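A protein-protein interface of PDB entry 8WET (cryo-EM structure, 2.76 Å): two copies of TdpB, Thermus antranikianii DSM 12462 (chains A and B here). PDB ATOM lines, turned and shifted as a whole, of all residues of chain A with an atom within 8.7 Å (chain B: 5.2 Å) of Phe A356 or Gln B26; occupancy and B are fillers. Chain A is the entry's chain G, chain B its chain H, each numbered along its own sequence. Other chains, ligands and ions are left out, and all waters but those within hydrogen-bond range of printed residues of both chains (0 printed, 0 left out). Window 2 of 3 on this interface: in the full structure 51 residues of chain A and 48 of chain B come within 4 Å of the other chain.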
ATOM      1  N   LEU A  75      14.763   6.280 -10.975  1.00  0.00           N
ATOM      2  CA  LEU A  75      15.900   7.087 -11.394  1.00  0.00           C
ATOM      3  C   LEU A  75      17.175   6.396 -10.937  1.00  0.00           C
ATOM      4  O   LEU A  75      17.281   5.998  -9.772  1.00  0.00           O
ATOM      5  CB  LEU A  75      15.823   8.502 -10.813  1.00  0.00           C
ATOM      6  CG  LEU A  75      14.831   9.481 -11.448  1.00  0.00           C
ATOM      7  CD1 LEU A  75      13.420   9.254 -10.928  1.00  0.00           C
ATOM      8  CD2 LEU A  75      15.272  10.910 -11.187  1.00  0.00           C
ATOM      9  N   GLU A 103      15.926  10.010 -17.561  1.00  0.00           N
ATOM     10  CA  GLU A 103      16.105  11.253 -18.308  1.00  0.00           C
ATOM     11  C   GLU A 103      17.130  11.090 -19.423  1.00  0.00           C
ATOM     12  O   GLU A 103      16.926  11.578 -20.540  1.00  0.00           O
ATOM     13  CB  GLU A 103      16.510  12.379 -17.354  1.00  0.00           C
ATOM     14  CG  GLU A 103      16.485  13.774 -17.967  1.00  0.00           C
ATOM     15  CD  GLU A 103      17.780  14.133 -18.668  1.00  0.00           C
ATOM     16  OE1 GLU A 103      18.840  13.620 -18.254  1.00  0.00           O
ATOM     17  OE2 GLU A 103      17.737  14.928 -19.630  1.00  0.00           O
ATOM     18  N   LEU A 349      19.208  10.471  -1.953  1.00  0.00           N
ATOM     19  CA  LEU A 349      18.970  11.706  -1.216  1.00  0.00           C
ATOM     20  C   LEU A 349      20.248  12.235  -0.577  1.00  0.00           C
ATOM     21  O   LEU A 349      20.410  13.454  -0.442  1.00  0.00           O
ATOM     22  CB  LEU A 349      17.892  11.497  -0.151  1.00  0.00           C
ATOM     23  CG  LEU A 349      16.434  11.696  -0.575  1.00  0.00           C
ATOM     24  CD1 LEU A 349      16.220  13.143  -0.990  1.00  0.00           C
ATOM     25  CD2 LEU A 349      16.012  10.745  -1.686  1.00  0.00           C
ATOM     26  N   ALA A 350      21.155  11.344  -0.172  1.00  0.00           N
ATOM     27  CA  ALA A 350      22.420  11.790   0.404  1.00  0.00           C
ATOM     28  C   ALA A 350      23.237  12.583  -0.607  1.00  0.00           C
ATOM     29  O   ALA A 350      23.798  13.634  -0.277  1.00  0.00           O
ATOM     30  CB  ALA A 350      23.215  10.590   0.916  1.00  0.00           C
ATOM     31  N   ARG A 351      23.316  12.095  -1.849  1.00  0.00           N
ATOM     32  CA  ARG A 351      24.050  12.823  -2.879  1.00  0.00           C
ATOM     33  C   ARG A 351      23.339  14.113  -3.263  1.00  0.00           C
ATOM     34  O   ARG A 351      23.988  15.142  -3.484  1.00  0.00           O
ATOM     35  CB  ARG A 351      24.252  11.938  -4.109  1.00  0.00           C
ATOM     36  CG  ARG A 351      25.161  10.749  -3.869  1.00  0.00           C
ATOM     37  CD  ARG A 351      26.534  11.199  -3.405  1.00  0.00           C
ATOM     38  NE  ARG A 351      27.458  10.079  -3.277  1.00  0.00           N
ATOM     39  CZ  ARG A 351      28.287   9.682  -4.233  1.00  0.00           C
ATOM     40  NH1 ARG A 351      28.339  10.298  -5.403  1.00  0.00           N
ATOM     41  NH2 ARG A 351      29.083   8.640  -4.009  1.00  0.00           N
ATOM     42  N   PHE A 352      22.008  14.081  -3.350  1.00  0.00           N
ATOM     43  CA  PHE A 352      21.268  15.278  -3.732  1.00  0.00           C
ATOM     44  C   PHE A 352      21.316  16.340  -2.641  1.00  0.00           C
ATOM     45  O   PHE A 352      21.247  17.537  -2.940  1.00  0.00           O
ATOM     46  CB  PHE A 352      19.821  14.918  -4.066  1.00  0.00           C
ATOM     47  CG  PHE A 352      19.123  15.936  -4.921  1.00  0.00           C
ATOM     48  CD1 PHE A 352      19.439  16.066  -6.262  1.00  0.00           C
ATOM     49  CD2 PHE A 352      18.148  16.761  -4.384  1.00  0.00           C
ATOM     50  CE1 PHE A 352      18.799  17.001  -7.052  1.00  0.00           C
ATOM     51  CE2 PHE A 352      17.504  17.697  -5.169  1.00  0.00           C
ATOM     52  CZ  PHE A 352      17.830  17.818  -6.505  1.00  0.00           C
ATOM     53  N   ARG A 353      21.427  15.924  -1.377  1.00  0.00           N
ATOM     54  CA  ARG A 353      21.557  16.889  -0.290  1.00  0.00           C
ATOM     55  C   ARG A 353      22.936  17.537  -0.284  1.00  0.00           C
ATOM     56  O   ARG A 353      23.054  18.757  -0.126  1.00  0.00           O
ATOM     57  CB  ARG A 353      21.275  16.210   1.051  1.00  0.00           C
ATOM     58  CG  ARG A 353      21.572  17.072   2.267  1.00  0.00           C
ATOM     59  CD  ARG A 353      20.711  18.324   2.289  1.00  0.00           C
ATOM     60  NE  ARG A 353      20.830  19.043   3.551  1.00  0.00           N
ATOM     61  CZ  ARG A 353      21.765  19.946   3.814  1.00  0.00           C
ATOM     62  NH1 ARG A 353      22.684  20.270   2.919  1.00  0.00           N
ATOM     63  NH2 ARG A 353      21.779  20.538   5.005  1.00  0.00           N
ATOM     64  N   LYS A 354      23.991  16.738  -0.459  1.00  0.00           N
ATOM     65  CA  LYS A 354      25.348  17.269  -0.441  1.00  0.00           C
ATOM     66  C   LYS A 354      25.712  17.998  -1.726  1.00  0.00           C
ATOM     67  O   LYS A 354      26.706  18.733  -1.745  1.00  0.00           O
ATOM     68  CB  LYS A 354      26.352  16.140  -0.187  1.00  0.00           C
ATOM     69  CG  LYS A 354      26.460  15.138  -1.324  1.00  0.00           C
ATOM     70  CD  LYS A 354      27.443  14.027  -0.990  1.00  0.00           C
ATOM     71  CE  LYS A 354      28.864  14.557  -0.896  1.00  0.00           C
ATOM     72  NZ  LYS A 354      29.318  15.152  -2.183  1.00  0.00           N
ATOM     73  N   ALA A 355      24.937  17.815  -2.790  1.00  0.00           N
ATOM     74  CA  ALA A 355      25.168  18.511  -4.048  1.00  0.00           C
ATOM     75  C   ALA A 355      24.537  19.901  -3.982  1.00  0.00           C
ATOM     76  O   ALA A 355      24.184  20.403  -2.911  1.00  0.00           O
ATOM     77  CB  ALA A 355      24.629  17.694  -5.218  1.00  0.00           C
ATOM     78  N   PHE A 356      24.410  20.545  -5.142  1.00  0.00           N
ATOM     79  CA  PHE A 356      23.821  21.874  -5.254  1.00  0.00           C
ATOM     80  C   PHE A 356      22.440  21.946  -4.610  1.00  0.00           C
ATOM     81  O   PHE A 356      21.762  20.925  -4.456  1.00  0.00           O
ATOM     82  CB  PHE A 356      23.726  22.283  -6.727  1.00  0.00           C
ATOM     83  CG  PHE A 356      22.732  21.477  -7.517  1.00  0.00           C
ATOM     84  CD1 PHE A 356      23.078  20.238  -8.033  1.00  0.00           C
ATOM     85  CD2 PHE A 356      21.452  21.958  -7.744  1.00  0.00           C
ATOM     86  CE1 PHE A 356      22.165  19.494  -8.757  1.00  0.00           C
ATOM     87  CE2 PHE A 356      20.536  21.217  -8.466  1.00  0.00           C
ATOM     88  CZ  PHE A 356      20.894  19.985  -8.974  1.00  0.00           C
ATOM     89  N   GLY A 357      22.019  23.151  -4.237  1.00  0.00           N
ATOM     90  CA  GLY A 357      20.721  23.345  -3.621  1.00  0.00           C
ATOM     91  C   GLY A 357      20.752  23.277  -2.109  1.00  0.00           C
ATOM     92  O   GLY A 357      20.534  24.289  -1.436  1.00  0.00           O
ATOM     93  N   GLU A 358      20.996  22.083  -1.567  1.00  0.00           N
ATOM     94  CA  GLU A 358      21.068  21.781  -0.140  1.00  0.00           C
ATOM     95  C   GLU A 358      19.715  21.908   0.550  1.00  0.00           C
ATOM     96  O   GLU A 358      19.612  21.612   1.747  1.00  0.00           O
ATOM     97  CB  GLU A 358      22.092  22.657   0.597  1.00  0.00           C
ATOM     98  CG  GLU A 358      23.535  22.366   0.218  1.00  0.00           C
ATOM     99  CD  GLU A 358      24.519  23.269   0.936  1.00  0.00           C
ATOM    100  OE1 GLU A 358      24.084  24.302   1.488  1.00  0.00           O
ATOM    101  OE2 GLU A 358      25.724  22.943   0.951  1.00  0.00           O
ATOM    102  N   ASP A 359      18.673  22.335  -0.163  1.00  0.00           N
ATOM    103  CA  ASP A 359      17.316  22.362   0.359  1.00  0.00           C
ATOM    104  C   ASP A 359      16.299  21.793  -0.616  1.00  0.00           C
ATOM    105  O   ASP A 359      15.144  21.589  -0.224  1.00  0.00           O
ATOM    106  CB  ASP A 359      16.906  23.795   0.733  1.00  0.00           C
ATOM    107  CG  ASP A 359      16.013  23.844   1.958  1.00  0.00           C
ATOM    108  OD1 ASP A 359      15.603  22.768   2.440  1.00  0.00           O
ATOM    109  OD2 ASP A 359      15.722  24.960   2.439  1.00  0.00           O
ATOM    110  N   LEU A 360      16.685  21.539  -1.869  1.00  0.00           N
ATOM    111  CA  LEU A 360      15.794  20.865  -2.804  1.00  0.00           C
ATOM    112  C   LEU A 360      15.563  19.417  -2.397  1.00  0.00           C
ATOM    113  O   LEU A 360      14.521  18.839  -2.728  1.00  0.00           O
ATOM    114  CB  LEU A 360      16.371  20.930  -4.218  1.00  0.00           C
ATOM    115  CG  LEU A 360      17.062  22.233  -4.624  1.00  0.00           C
ATOM    116  CD1 LEU A 360      17.713  22.085  -5.990  1.00  0.00           C
ATOM    117  CD2 LEU A 360      16.084  23.395  -4.619  1.00  0.00           C
ATOM    118  N   ALA A 361      16.522  18.818  -1.687  1.00  0.00           N
ATOM    119  CA  ALA A 361      16.343  17.459  -1.192  1.00  0.00           C
ATOM    120  C   ALA A 361      15.198  17.388  -0.189  1.00  0.00           C
ATOM    121  O   ALA A 361      14.421  16.427  -0.191  1.00  0.00           O
ATOM    122  CB  ALA A 361      17.641  16.952  -0.566  1.00  0.00           C
ATOM    123  N   LYS A 363      12.558  19.258  -0.188  1.00  0.00           N
ATOM    124  CA  LYS A 363      11.352  19.263  -1.009  1.00  0.00           C
ATOM    125  C   LYS A 363      11.126  17.904  -1.660  1.00  0.00           C
ATOM    126  O   LYS A 363       9.985  17.439  -1.757  1.00  0.00           O
ATOM    127  CB  LYS A 363      11.443  20.356  -2.072  1.00  0.00           C
ATOM    128  CG  LYS A 363      11.276  21.767  -1.537  1.00  0.00           C
ATOM    129  CD  LYS A 363      11.300  22.784  -2.667  1.00  0.00           C
ATOM    130  CE  LYS A 363      12.687  22.900  -3.275  1.00  0.00           C
ATOM    131  NZ  LYS A 363      12.762  23.992  -4.283  1.00  0.00           N
ATOM    132  N   LEU A 364      12.202  17.255  -2.111  1.00  0.00           N
ATOM    133  CA  LEU A 364      12.067  15.971  -2.791  1.00  0.00           C
ATOM    134  C   LEU A 364      11.521  14.903  -1.850  1.00  0.00           C
ATOM    135  O   LEU A 364      10.718  14.057  -2.262  1.00  0.00           O
ATOM    136  CB  LEU A 364      13.419  15.554  -3.378  1.00  0.00           C
ATOM    137  CG  LEU A 364      13.508  14.340  -4.310  1.00  0.00           C
ATOM    138  CD1 LEU A 364      14.682  14.509  -5.257  1.00  0.00           C
ATOM    139  CD2 LEU A 364      13.649  13.039  -3.540  1.00  0.00           C
ATOM    140  N   ASP B  23      24.192  13.800 -13.782  1.00  0.00           N
ATOM    141  CA  ASP B  23      24.346  14.872 -14.757  1.00  0.00           C
ATOM    142  C   ASP B  23      23.498  16.090 -14.410  1.00  0.00           C
ATOM    143  O   ASP B  23      24.043  17.179 -14.209  1.00  0.00           O
ATOM    144  CB  ASP B  23      24.010  14.356 -16.166  1.00  0.00           C
ATOM    145  CG  ASP B  23      22.632  13.726 -16.249  1.00  0.00           C
ATOM    146  OD1 ASP B  23      22.209  13.086 -15.264  1.00  0.00           O
ATOM    147  OD2 ASP B  23      21.972  13.878 -17.298  1.00  0.00           O
ATOM    148  N   HIS B  24      22.176  15.935 -14.320  1.00  0.00           N
ATOM    149  CA  HIS B  24      21.300  17.016 -13.885  1.00  0.00           C
ATOM    150  C   HIS B  24      19.916  16.487 -13.523  1.00  0.00           C
ATOM    151  O   HIS B  24      19.237  15.879 -14.356  1.00  0.00           O
ATOM    152  CB  HIS B  24      21.197  18.100 -14.965  1.00  0.00           C
ATOM    153  CG  HIS B  24      20.648  17.612 -16.269  1.00  0.00           C
ATOM    154  ND1 HIS B  24      19.318  17.739 -16.610  1.00  0.00           N
ATOM    155  CD2 HIS B  24      21.247  16.999 -17.316  1.00  0.00           C
ATOM    156  CE1 HIS B  24      19.123  17.225 -17.810  1.00  0.00           C
ATOM    157  NE2 HIS B  24      20.277  16.769 -18.261  1.00  0.00           N
ATOM    158  N   TYR B  25      19.493  16.712 -12.280  1.00  0.00           N
ATOM    159  CA  TYR B  25      18.146  16.377 -11.840  1.00  0.00           C
ATOM    160  C   TYR B  25      17.343  17.593 -11.405  1.00  0.00           C
ATOM    161  O   TYR B  25      16.189  17.435 -10.990  1.00  0.00           O
ATOM    162  CB  TYR B  25      18.185  15.359 -10.691  1.00  0.00           C
ATOM    163  CG  TYR B  25      18.561  13.954 -11.110  1.00  0.00           C
ATOM    164  CD1 TYR B  25      18.545  13.577 -12.446  1.00  0.00           C
ATOM    165  CD2 TYR B  25      18.919  13.002 -10.165  1.00  0.00           C
ATOM    166  CE1 TYR B  25      18.884  12.294 -12.830  1.00  0.00           C
ATOM    167  CE2 TYR B  25      19.259  11.716 -10.540  1.00  0.00           C
ATOM    168  CZ  TYR B  25      19.240  11.368 -11.873  1.00  0.00           C
ATOM    169  OH  TYR B  25      19.577  10.088 -12.250  1.00  0.00           O
ATOM    170  N   GLN B  26      17.915  18.797 -11.483  1.00  0.00           N
ATOM    171  CA  GLN B  26      17.182  19.997 -11.099  1.00  0.00           C
ATOM    172  C   GLN B  26      16.041  20.308 -12.057  1.00  0.00           C
ATOM    173  O   GLN B  26      15.081  20.977 -11.662  1.00  0.00           O
ATOM    174  CB  GLN B  26      18.131  21.194 -11.009  1.00  0.00           C
ATOM    175  CG  GLN B  26      18.550  21.773 -12.352  1.00  0.00           C
ATOM    176  CD  GLN B  26      19.749  21.059 -12.949  1.00  0.00           C
ATOM    177  OE1 GLN B  26      20.092  19.950 -12.542  1.00  0.00           O
ATOM    178  NE2 GLN B  26      20.394  21.697 -13.919  1.00  0.00           N
ATOM    179  N   ASP B  27      16.122  19.839 -13.304  1.00  0.00           N
ATOM    180  CA  ASP B  27      15.056  20.102 -14.264  1.00  0.00           C
ATOM    181  C   ASP B  27      13.794  19.314 -13.940  1.00  0.00           C
ATOM    182  O   ASP B  27      12.685  19.797 -14.194  1.00  0.00           O
ATOM    183  CB  ASP B  27      15.531  19.778 -15.680  1.00  0.00           C
ATOM    184  CG  ASP B  27      16.146  18.394 -15.785  1.00  0.00           C
ATOM    185  OD1 ASP B  27      16.621  17.872 -14.755  1.00  0.00           O
ATOM    186  OD2 ASP B  27      16.152  17.829 -16.900  1.00  0.00           O
ATOM    187  N   LEU B  28      13.940  18.110 -13.382  1.00  0.00           N
ATOM    188  CA  LEU B  28      12.784  17.241 -13.181  1.00  0.00           C
ATOM    189  C   LEU B  28      11.814  17.827 -12.160  1.00  0.00           C
ATOM    190  O   LEU B  28      10.611  17.931 -12.426  1.00  0.00           O
ATOM    191  CB  LEU B  28      13.247  15.848 -12.757  1.00  0.00           C
ATOM    192  CG  LEU B  28      14.226  15.168 -13.715  1.00  0.00           C
ATOM    193  CD1 LEU B  28      14.446  13.716 -13.326  1.00  0.00           C
ATOM    194  CD2 LEU B  28      13.733  15.269 -15.152  1.00  0.00           C
ATOM    195  N   LEU B  29      12.315  18.224 -10.987  1.00  0.00           N
ATOM    196  CA  LEU B  29      11.431  18.817  -9.990  1.00  0.00           C
ATOM    197  C   LEU B  29      11.051  20.249 -10.342  1.00  0.00           C
ATOM    198  O   LEU B  29      10.050  20.755  -9.824  1.00  0.00           O
ATOM    199  CB  LEU B  29      12.060  18.774  -8.595  1.00  0.00           C
ATOM    200  CG  LEU B  29      13.215  19.712  -8.236  1.00  0.00           C
ATOM    201  CD1 LEU B  29      13.393  19.760  -6.728  1.00  0.00           C
ATOM    202  CD2 LEU B  29      14.501  19.262  -8.890  1.00  0.00           C
ATOM    203  N   ARG B  30      11.830  20.915 -11.199  1.00  0.00           N
ATOM    204  CA  ARG B  30      11.417  22.219 -11.706  1.00  0.00           C
ATOM    205  C   ARG B  30      10.137  22.098 -12.522  1.00  0.00           C
ATOM    206  O   ARG B  30       9.224  22.921 -12.389  1.00  0.00           O
ATOM    207  CB  ARG B  30      12.536  22.841 -12.542  1.00  0.00           C
ATOM    208  CG  ARG B  30      12.130  24.102 -13.289  1.00  0.00           C
ATOM    209  CD  ARG B  30      12.885  24.250 -14.603  1.00  0.00           C
ATOM    210  NE  ARG B  30      14.324  24.389 -14.415  1.00  0.00           N
ATOM    211  CZ  ARG B  30      15.236  23.813 -15.186  1.00  0.00           C
ATOM    212  NH1 ARG B  30      14.890  23.054 -16.214  1.00  0.00           N
ATOM    213  NH2 ARG B  30      16.525  24.004 -14.922  1.00  0.00           N
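No position is printed for both chains.
Hydrophobic or aromatic side chains of chain A within 4 Å of the printed part of chain B: Leu A75 and Phe A356. Printed residues of chain B that touch a printed residue of chain A: Asp B23, His B24, Gln B26 and Leu B28. Hydrophobic or aromatic side chains of chain B that line the printed part of chain A: His B24 and Leu B28. Among the printed residues, 4 pairs touch across the chains.
Among the printed residues, merely in contact across the chains: Leu A75 with Leu B28 (3.6 Å) and Phe A356 with Gln B26 (3.5 Å).
A ring nitrogen (NE2) of His B24 sits close to the side-chain carboxylate of Glu A103 (3.4 Å). The side-chain carboxylate of Glu A103 lies close to the side-chain carboxylate of Asp B23.
The side-chain carboxylate of Asp B23 sits close to a ring nitrogen (NE2) of His B24, at 3.5 Å. ND1 of His B24 lies close to OD2 of Asp B27 (3.2 Å).
Phe A356 touches one residue of chain B. Gln B26 touches just one residue of chain A: Phe A356 (3.5 Å). Printed residues of chain B within 4 Å of Glu A103: Asp B23 and His B24. Printed residues of chain A within 4 Å of His B24: Glu A103 (3.2 Å). Printed residues of chain A within 4 Å of Leu B28: Leu A75. Printed residues of chain A within 4 Å of Asp B23: Glu A103. Glu A358 touches none of the printed residues of chain B. Ala A355 touches none of the printed residues of chain B. The nearest residue of chain B that does not touch Phe A356 is Tyr B25 (4.9 Å).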
